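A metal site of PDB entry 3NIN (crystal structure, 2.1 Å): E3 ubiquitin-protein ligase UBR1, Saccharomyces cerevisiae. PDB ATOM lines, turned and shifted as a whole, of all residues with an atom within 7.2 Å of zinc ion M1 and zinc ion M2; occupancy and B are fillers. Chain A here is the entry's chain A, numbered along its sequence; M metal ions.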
ATOM      1  N   HIS A   4     -24.395   9.305  12.680  1.00  0.00           N
ATOM      2  CA  HIS A   4     -23.974   7.955  12.320  1.00  0.00           C
ATOM      3  C   HIS A   4     -24.598   7.482  10.999  1.00  0.00           C
ATOM      4  O   HIS A   4     -24.425   6.329  10.582  1.00  0.00           O
ATOM      5  CB  HIS A   4     -24.296   6.968  13.450  1.00  0.00           C
ATOM      6  CG  HIS A   4     -23.777   7.389  14.791  1.00  0.00           C
ATOM      7  ND1 HIS A   4     -22.425   7.392  15.100  1.00  0.00           N
ATOM      8  CD2 HIS A   4     -24.414   7.808  15.915  1.00  0.00           C
ATOM      9  CE1 HIS A   4     -22.265   7.800  16.355  1.00  0.00           C
ATOM     10  NE2 HIS A   4     -23.452   8.044  16.864  1.00  0.00           N
ATOM     11  N   LYS A   5     -25.312   8.387  10.335  1.00  0.00           N
ATOM     12  CA  LYS A   5     -25.890   8.133   9.019  1.00  0.00           C
ATOM     13  C   LYS A   5     -24.799   7.888   7.977  1.00  0.00           C
ATOM     14  O   LYS A   5     -23.783   8.582   7.942  1.00  0.00           O
ATOM     15  CB  LYS A   5     -26.734   9.313   8.551  1.00  0.00           C
ATOM     16  CG  LYS A   5     -28.066   9.467   9.275  1.00  0.00           C
ATOM     17  CD  LYS A   5     -28.944  10.543   8.632  1.00  0.00           C
ATOM     18  CE  LYS A   5     -29.517  10.093   7.297  1.00  0.00           C
ATOM     19  NZ  LYS A   5     -30.391  11.138   6.682  1.00  0.00           N
ATOM     20  N   HIS A   6     -25.017   6.880   7.124  1.00  0.00           N
ATOM     21  CA  HIS A   6     -24.104   6.591   6.024  1.00  0.00           C
ATOM     22  C   HIS A   6     -24.877   6.249   4.741  1.00  0.00           C
ATOM     23  O   HIS A   6     -24.507   5.321   4.018  1.00  0.00           O
ATOM     24  CB  HIS A   6     -23.154   5.455   6.422  1.00  0.00           C
ATOM     25  CG  HIS A   6     -23.843   4.161   6.702  1.00  0.00           C
ATOM     26  ND1 HIS A   6     -24.211   3.292   5.694  1.00  0.00           N
ATOM     27  CD2 HIS A   6     -24.256   3.597   7.859  1.00  0.00           C
ATOM     28  CE1 HIS A   6     -24.819   2.242   6.226  1.00  0.00           C
ATOM     29  NE2 HIS A   6     -24.848   2.401   7.535  1.00  0.00           N
ATOM     30  N   ARG A   9     -23.953   4.192   1.133  1.00  0.00           N
ATOM     31  CA  ARG A   9     -22.722   3.412   1.254  1.00  0.00           C
ATOM     32  C   ARG A   9     -22.763   2.485   2.458  1.00  0.00           C
ATOM     33  O   ARG A   9     -23.754   2.441   3.174  1.00  0.00           O
ATOM     34  CB  ARG A   9     -21.476   4.319   1.299  1.00  0.00           C
ATOM     35  CG  ARG A   9     -21.477   5.378   2.407  1.00  0.00           C
ATOM     36  CD  ARG A   9     -20.057   5.826   2.770  1.00  0.00           C
ATOM     37  NE  ARG A   9     -19.494   4.993   3.842  1.00  0.00           N
ATOM     38  CZ  ARG A   9     -18.371   5.244   4.511  1.00  0.00           C
ATOM     39  NH1 ARG A   9     -17.640   6.311   4.227  1.00  0.00           N
ATOM     40  NH2 ARG A   9     -17.973   4.404   5.470  1.00  0.00           N
ATOM     41  N   ASN A  10     -21.703   1.724   2.674  1.00  0.00           N
ATOM     42  CA  ASN A  10     -21.612   0.881   3.860  1.00  0.00           C
ATOM     43  C   ASN A  10     -21.268   1.725   5.088  1.00  0.00           C
ATOM     44  O   ASN A  10     -20.767   2.848   4.960  1.00  0.00           O
ATOM     45  CB  ASN A  10     -20.560  -0.217   3.680  1.00  0.00           C
ATOM     46  CG  ASN A  10     -19.160   0.341   3.518  1.00  0.00           C
ATOM     47  OD1 ASN A  10     -18.923   1.221   2.694  1.00  0.00           O
ATOM     48  ND2 ASN A  10     -18.224  -0.175   4.312  1.00  0.00           N
ATOM     49  N   CYS A  11     -21.524   1.178   6.266  1.00  0.00           N
ATOM     50  CA  CYS A  11     -21.116   1.812   7.508  1.00  0.00           C
ATOM     51  C   CYS A  11     -19.604   1.743   7.705  1.00  0.00           C
ATOM     52  O   CYS A  11     -18.926   2.774   7.834  1.00  0.00           O
ATOM     53  CB  CYS A  11     -21.821   1.194   8.705  1.00  0.00           C
ATOM     54  SG  CYS A  11     -21.094   1.749  10.222  1.00  0.00           S
ATOM     55  N   GLY A  12     -19.068   0.521   7.751  1.00  0.00           N
ATOM     56  CA  GLY A  12     -17.628   0.294   7.824  1.00  0.00           C
ATOM     57  C   GLY A  12     -16.930   0.791   9.078  1.00  0.00           C
ATOM     58  O   GLY A  12     -15.703   0.916   9.093  1.00  0.00           O
ATOM     59  N   ARG A  13     -17.703   1.077  10.124  1.00  0.00           N
ATOM     60  CA  ARG A  13     -17.142   1.493  11.410  1.00  0.00           C
ATOM     61  C   ARG A  13     -16.272   0.381  11.962  1.00  0.00           C
ATOM     62  O   ARG A  13     -16.741  -0.743  12.150  1.00  0.00           O
ATOM     63  CB  ARG A  13     -18.240   1.846  12.425  1.00  0.00           C
ATOM     64  CG  ARG A  13     -17.698   2.173  13.816  1.00  0.00           C
ATOM     65  CD  ARG A  13     -18.797   2.463  14.834  1.00  0.00           C
ATOM     66  NE  ARG A  13     -19.140   3.889  14.875  1.00  0.00           N
ATOM     67  CZ  ARG A  13     -18.561   4.784  15.674  1.00  0.00           C
ATOM     68  NH1 ARG A  13     -17.602   4.413  16.509  1.00  0.00           N
ATOM     69  NH2 ARG A  13     -18.951   6.051  15.628  1.00  0.00           N
ATOM     70  N   PHE A  15     -14.415  -1.457  14.843  1.00  0.00           N
ATOM     71  CA  PHE A  15     -14.686  -1.617  16.263  1.00  0.00           C
ATOM     72  C   PHE A  15     -13.458  -1.312  17.097  1.00  0.00           C
ATOM     73  O   PHE A  15     -12.320  -1.545  16.669  1.00  0.00           O
ATOM     74  CB  PHE A  15     -15.227  -3.014  16.538  1.00  0.00           C
ATOM     75  CG  PHE A  15     -16.598  -3.247  15.952  1.00  0.00           C
ATOM     76  CD1 PHE A  15     -17.728  -2.744  16.595  1.00  0.00           C
ATOM     77  CD2 PHE A  15     -16.742  -3.946  14.764  1.00  0.00           C
ATOM     78  CE1 PHE A  15     -18.995  -2.935  16.043  1.00  0.00           C
ATOM     79  CE2 PHE A  15     -18.011  -4.154  14.214  1.00  0.00           C
ATOM     80  CZ  PHE A  15     -19.141  -3.651  14.857  1.00  0.00           C
ATOM     81  N   VAL A  34     -21.401  -8.673  10.950  1.00  0.00           N
ATOM     82  CA  VAL A  34     -21.687  -7.953  12.206  1.00  0.00           C
ATOM     83  C   VAL A  34     -22.248  -6.548  11.985  1.00  0.00           C
ATOM     84  O   VAL A  34     -22.083  -5.966  10.912  1.00  0.00           O
ATOM     85  CB  VAL A  34     -20.440  -7.859  13.131  1.00  0.00           C
ATOM     86  CG1 VAL A  34     -20.061  -9.236  13.672  1.00  0.00           C
ATOM     87  CG2 VAL A  34     -19.258  -7.202  12.405  1.00  0.00           C
ATOM     88  N   LEU A  35     -22.891  -6.011  13.029  1.00  0.00           N
ATOM     89  CA  LEU A  35     -23.486  -4.660  13.029  1.00  0.00           C
ATOM     90  C   LEU A  35     -23.057  -3.887  14.275  1.00  0.00           C
ATOM     91  O   LEU A  35     -23.071  -4.439  15.373  1.00  0.00           O
ATOM     92  CB  LEU A  35     -25.020  -4.772  13.025  1.00  0.00           C
ATOM     93  CG  LEU A  35     -25.720  -5.304  11.776  1.00  0.00           C
ATOM     94  CD1 LEU A  35     -27.198  -5.525  12.025  1.00  0.00           C
ATOM     95  CD2 LEU A  35     -25.512  -4.359  10.602  1.00  0.00           C
ATOM     96  N   CYS A  36     -22.706  -2.612  14.121  1.00  0.00           N
ATOM     97  CA  CYS A  36     -22.451  -1.757  15.289  1.00  0.00           C
ATOM     98  C   CYS A  36     -23.769  -1.377  16.009  1.00  0.00           C
ATOM     99  O   CYS A  36     -24.847  -1.680  15.500  1.00  0.00           O
ATOM    100  CB  CYS A  36     -21.660  -0.506  14.894  1.00  0.00           C
ATOM    101  SG  CYS A  36     -22.635   0.776  14.067  1.00  0.00           S
ATOM    102  N   ILE A  37     -23.685  -0.719  17.160  1.00  0.00           N
ATOM    103  CA  ILE A  37     -24.884  -0.310  17.919  1.00  0.00           C
ATOM    104  C   ILE A  37     -25.702   0.800  17.263  1.00  0.00           C
ATOM    105  O   ILE A  37     -26.913   0.892  17.467  1.00  0.00           O
ATOM    106  CB  ILE A  37     -24.597   0.105  19.389  1.00  0.00           C
ATOM    107  CG1 ILE A  37     -23.441   1.102  19.471  1.00  0.00           C
ATOM    108  CG2 ILE A  37     -24.387  -1.127  20.262  1.00  0.00           C
ATOM    109  CD1 ILE A  37     -23.455   1.955  20.735  1.00  0.00           C
ATOM    110  N   HIS A  38     -25.032   1.652  16.491  1.00  0.00           N
ATOM    111  CA  HIS A  38     -25.704   2.788  15.866  1.00  0.00           C
ATOM    112  C   HIS A  38     -26.519   2.330  14.650  1.00  0.00           C
ATOM    113  O   HIS A  38     -27.416   3.031  14.197  1.00  0.00           O
ATOM    114  CB  HIS A  38     -24.680   3.855  15.491  1.00  0.00           C
ATOM    115  CG  HIS A  38     -23.794   4.247  16.625  1.00  0.00           C
ATOM    116  ND1 HIS A  38     -22.440   3.975  16.648  1.00  0.00           N
ATOM    117  CD2 HIS A  38     -24.066   4.877  17.789  1.00  0.00           C
ATOM    118  CE1 HIS A  38     -21.911   4.423  17.773  1.00  0.00           C
ATOM    119  NE2 HIS A  38     -22.880   4.974  18.491  1.00  0.00           N
ATOM    120  N   CYS A  39     -26.215   1.127  14.171  1.00  0.00           N
ATOM    121  CA  CYS A  39     -26.830   0.587  12.966  1.00  0.00           C
ATOM    122  C   CYS A  39     -27.871  -0.499  13.236  1.00  0.00           C
ATOM    123  O   CYS A  39     -28.909  -0.554  12.563  1.00  0.00           O
ATOM    124  CB  CYS A  39     -25.739   0.081  12.027  1.00  0.00           C
ATOM    125  SG  CYS A  39     -24.775   1.407  11.204  1.00  0.00           S
ATOM    126  N   PHE A  40     -27.617  -1.377  14.203  1.00  0.00           N
ATOM    127  CA  PHE A  40     -28.538  -2.481  14.513  1.00  0.00           C
ATOM    128  C   PHE A  40     -29.954  -1.958  14.809  1.00  0.00           C
ATOM    129  O   PHE A  40     -30.157  -1.184  15.753  1.00  0.00           O
ATOM    130  CB  PHE A  40     -28.023  -3.350  15.667  1.00  0.00           C
ATOM    131  CG  PHE A  40     -28.992  -4.420  16.107  1.00  0.00           C
ATOM    132  CD1 PHE A  40     -29.001  -5.672  15.486  1.00  0.00           C
ATOM    133  CD2 PHE A  40     -29.893  -4.193  17.146  1.00  0.00           C
ATOM    134  CE1 PHE A  40     -29.883  -6.674  15.884  1.00  0.00           C
ATOM    135  CE2 PHE A  40     -30.803  -5.191  17.552  1.00  0.00           C
ATOM    136  CZ  PHE A  40     -30.791  -6.424  16.918  1.00  0.00           C
ATOM    137  N   ILE A  62     -15.076  -4.559  11.100  1.00  0.00           N
ATOM    138  CA  ILE A  62     -15.969  -3.435  10.777  1.00  0.00           C
ATOM    139  C   ILE A  62     -17.435  -3.846  10.655  1.00  0.00           C
ATOM    140  O   ILE A  62     -17.732  -4.981  10.297  1.00  0.00           O
ATOM    141  CB  ILE A  62     -15.546  -2.726   9.452  1.00  0.00           C
ATOM    142  CG1 ILE A  62     -15.765  -3.628   8.227  1.00  0.00           C
ATOM    143  CG2 ILE A  62     -14.089  -2.206   9.517  1.00  0.00           C
ATOM    144  CD1 ILE A  62     -15.494  -2.949   6.876  1.00  0.00           C
ATOM    145  N   CYS A  63     -18.327  -2.893  10.950  1.00  0.00           N
ATOM    146  CA  CYS A  63     -19.765  -3.022  10.766  1.00  0.00           C
ATOM    147  C   CYS A  63     -20.096  -3.235   9.283  1.00  0.00           C
ATOM    148  O   CYS A  63     -19.572  -2.553   8.414  1.00  0.00           O
ATOM    149  CB  CYS A  63     -20.484  -1.773  11.328  1.00  0.00           C
ATOM    150  SG  CYS A  63     -22.291  -1.540  11.053  1.00  0.00           S
ATOM    151  N   ASP A  64     -20.984  -4.197   9.002  1.00  0.00           N
ATOM    152  CA  ASP A  64     -21.366  -4.547   7.639  1.00  0.00           C
ATOM    153  C   ASP A  64     -22.692  -3.924   7.174  1.00  0.00           C
ATOM    154  O   ASP A  64     -23.148  -4.223   6.079  1.00  0.00           O
ATOM    155  CB  ASP A  64     -21.454  -6.072   7.478  1.00  0.00           C
ATOM    156  CG  ASP A  64     -20.112  -6.765   7.715  1.00  0.00           C
ATOM    157  OD1 ASP A  64     -19.191  -6.568   6.913  1.00  0.00           O
ATOM    158  OD2 ASP A  64     -20.010  -7.527   8.691  1.00  0.00           O
ATOM    159  N   CYS A  65     -23.314  -3.095   8.020  1.00  0.00           N
ATOM    160  CA  CYS A  65     -24.542  -2.363   7.643  1.00  0.00           C
ATOM    161  C   CYS A  65     -24.315  -1.649   6.305  1.00  0.00           C
ATOM    162  O   CYS A  65     -23.383  -0.862   6.161  1.00  0.00           O
ATOM    163  CB  CYS A  65     -24.946  -1.356   8.735  1.00  0.00           C
ATOM    164  SG  CYS A  65     -26.404  -0.255   8.417  1.00  0.00           S
ATOM    165  N   GLY A  66     -25.158  -1.971   5.318  1.00  0.00           N
ATOM    166  CA  GLY A  66     -25.046  -1.381   3.973  1.00  0.00           C
ATOM    167  C   GLY A  66     -24.209  -2.171   2.974  1.00  0.00           C
ATOM    168  O   GLY A  66     -24.101  -1.777   1.815  1.00  0.00           O
ATOM    169  N   HIS A  76     -32.594  -2.242   7.455  1.00  0.00           N
ATOM    170  CA  HIS A  76     -33.081  -0.873   7.567  1.00  0.00           C
ATOM    171  C   HIS A  76     -32.335  -0.183   8.690  1.00  0.00           C
ATOM    172  O   HIS A  76     -32.648  -0.362   9.860  1.00  0.00           O
ATOM    173  CB  HIS A  76     -34.593  -0.864   7.770  1.00  0.00           C
ATOM    174  CG  HIS A  76     -35.337  -1.633   6.719  1.00  0.00           C
ATOM    175  ND1 HIS A  76     -35.662  -2.965   6.858  1.00  0.00           N
ATOM    176  CD2 HIS A  76     -35.791  -1.260   5.492  1.00  0.00           C
ATOM    177  CE1 HIS A  76     -36.285  -3.374   5.778  1.00  0.00           C
ATOM    178  NE2 HIS A  76     -36.382  -2.365   4.939  1.00  0.00           N
ATOM    179  N   CYS A  77     -31.330   0.598   8.307  1.00  0.00           N
ATOM    180  CA  CYS A  77     -30.372   1.177   9.235  1.00  0.00           C
ATOM    181  C   CYS A  77     -31.039   2.063  10.290  1.00  0.00           C
ATOM    182  O   CYS A  77     -31.838   2.935   9.950  1.00  0.00           O
ATOM    183  CB  CYS A  77     -29.300   1.963   8.477  1.00  0.00           C
ATOM    184  SG  CYS A  77     -28.101   2.778   9.543  1.00  0.00           S
ATOM    185  N   LYS A  78     -30.705   1.824  11.554  1.00  0.00           N
ATOM    186  CA  LYS A  78     -31.271   2.569  12.671  1.00  0.00           C
ATOM    187  C   LYS A  78     -30.946   4.063  12.608  1.00  0.00           C
ATOM    188  O   LYS A  78     -31.786   4.898  12.935  1.00  0.00           O
ATOM    189  CB  LYS A  78     -30.812   1.994  14.014  1.00  0.00           C
ATOM    190  CG  LYS A  78     -31.431   2.688  15.230  1.00  0.00           C
ATOM    191  CD  LYS A  78     -31.416   1.806  16.455  1.00  0.00           C
ATOM    192  CE  LYS A  78     -31.347   2.636  17.736  1.00  0.00           C
ATOM    193  NZ  LYS A  78     -29.964   3.157  17.960  1.00  0.00           N
ATOM    194  N   ALA A  79     -29.721   4.372  12.179  1.00  0.00           N
ATOM    195  CA  ALA A  79     -29.270   5.756  12.039  1.00  0.00           C
ATOM    196  C   ALA A  79     -30.112   6.568  11.043  1.00  0.00           C
ATOM    197  O   ALA A  79     -30.141   7.799  11.113  1.00  0.00           O
ATOM    198  CB  ALA A  79     -27.791   5.807  11.664  1.00  0.00           C
ATOM    199  N   GLU A  80     -30.774   5.873  10.118  1.00  0.00           N
ATOM    200  CA  GLU A  80     -31.649   6.521   9.133  1.00  0.00           C
ATOM    201  C   GLU A  80     -32.937   7.062   9.775  1.00  0.00           C
ATOM    202  O   GLU A  80     -33.479   8.067   9.307  1.00  0.00           O
ATOM    203  CB  GLU A  80     -32.000   5.561   7.988  1.00  0.00           C
ATOM    204  CG  GLU A  80     -30.825   5.157   7.090  1.00  0.00           C
ATOM    205  CD  GLU A  80     -30.341   6.277   6.183  1.00  0.00           C
ATOM    206  OE1 GLU A  80     -31.079   7.268   5.979  1.00  0.00           O
ATOM    207  OE2 GLU A  80     -29.217   6.159   5.652  1.00  0.00           O
HETATM  208 ZN    ZN M   1     -22.522   0.531  11.746  1.00  0.00          ZN
HETATM  209 ZN    ZN M   2     -26.032   1.588   9.310  1.00  0.00          ZN
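The side-chain sulfur (SG) of Cys 63 sits close to the backbone NH (N) of Cys 65, 3.6 Å away. The backbone NH (N) of Cys 63 is in hydrogen-bond range of the backbone carbonyl oxygen (O) of Arg 13. N of Gly 12 is in hydrogen-bond range of O of Cys 63, 3.2 Å away. ND1 of His 6 sits at hydrogen-bond distance from O of Arg 9, at 2.7 Å. N of His 38 lies close to SG of Cys 36, 3.5 Å away. SG of Cys 77 sits close to N of Ala 79, at 3.5 Å. The side-chain sulfur (SG) of Cys 11 lies close to the backbone NH (N) of Arg 13 (3.5 Å). O of Cys 11 lies within hydrogen-bond range of NH2 of Arg 9.
Zinc ion M1 is bound by the side-chain sulfur (SG) of Cys 63, the side-chain sulfur (SG) of Cys 36, the side-chain sulfur (SG) of Cys 11 and the side-chain sulfur (SG) of Cys 39.
SG of Cys 65 binds zinc ion M2, at 2.1 Å. The side-chain sulfur (SG) of Cys 39 is bound to zinc ion M2 (2.3 Å). Zinc ion M2 is bound by NE2 of His 6. SG of Cys 77 is bound to zinc ion M2, at 2.4 Å.
Within 4 Å of zinc ion M2: His 6, Cys 39, Cys 65 and Cys 77.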
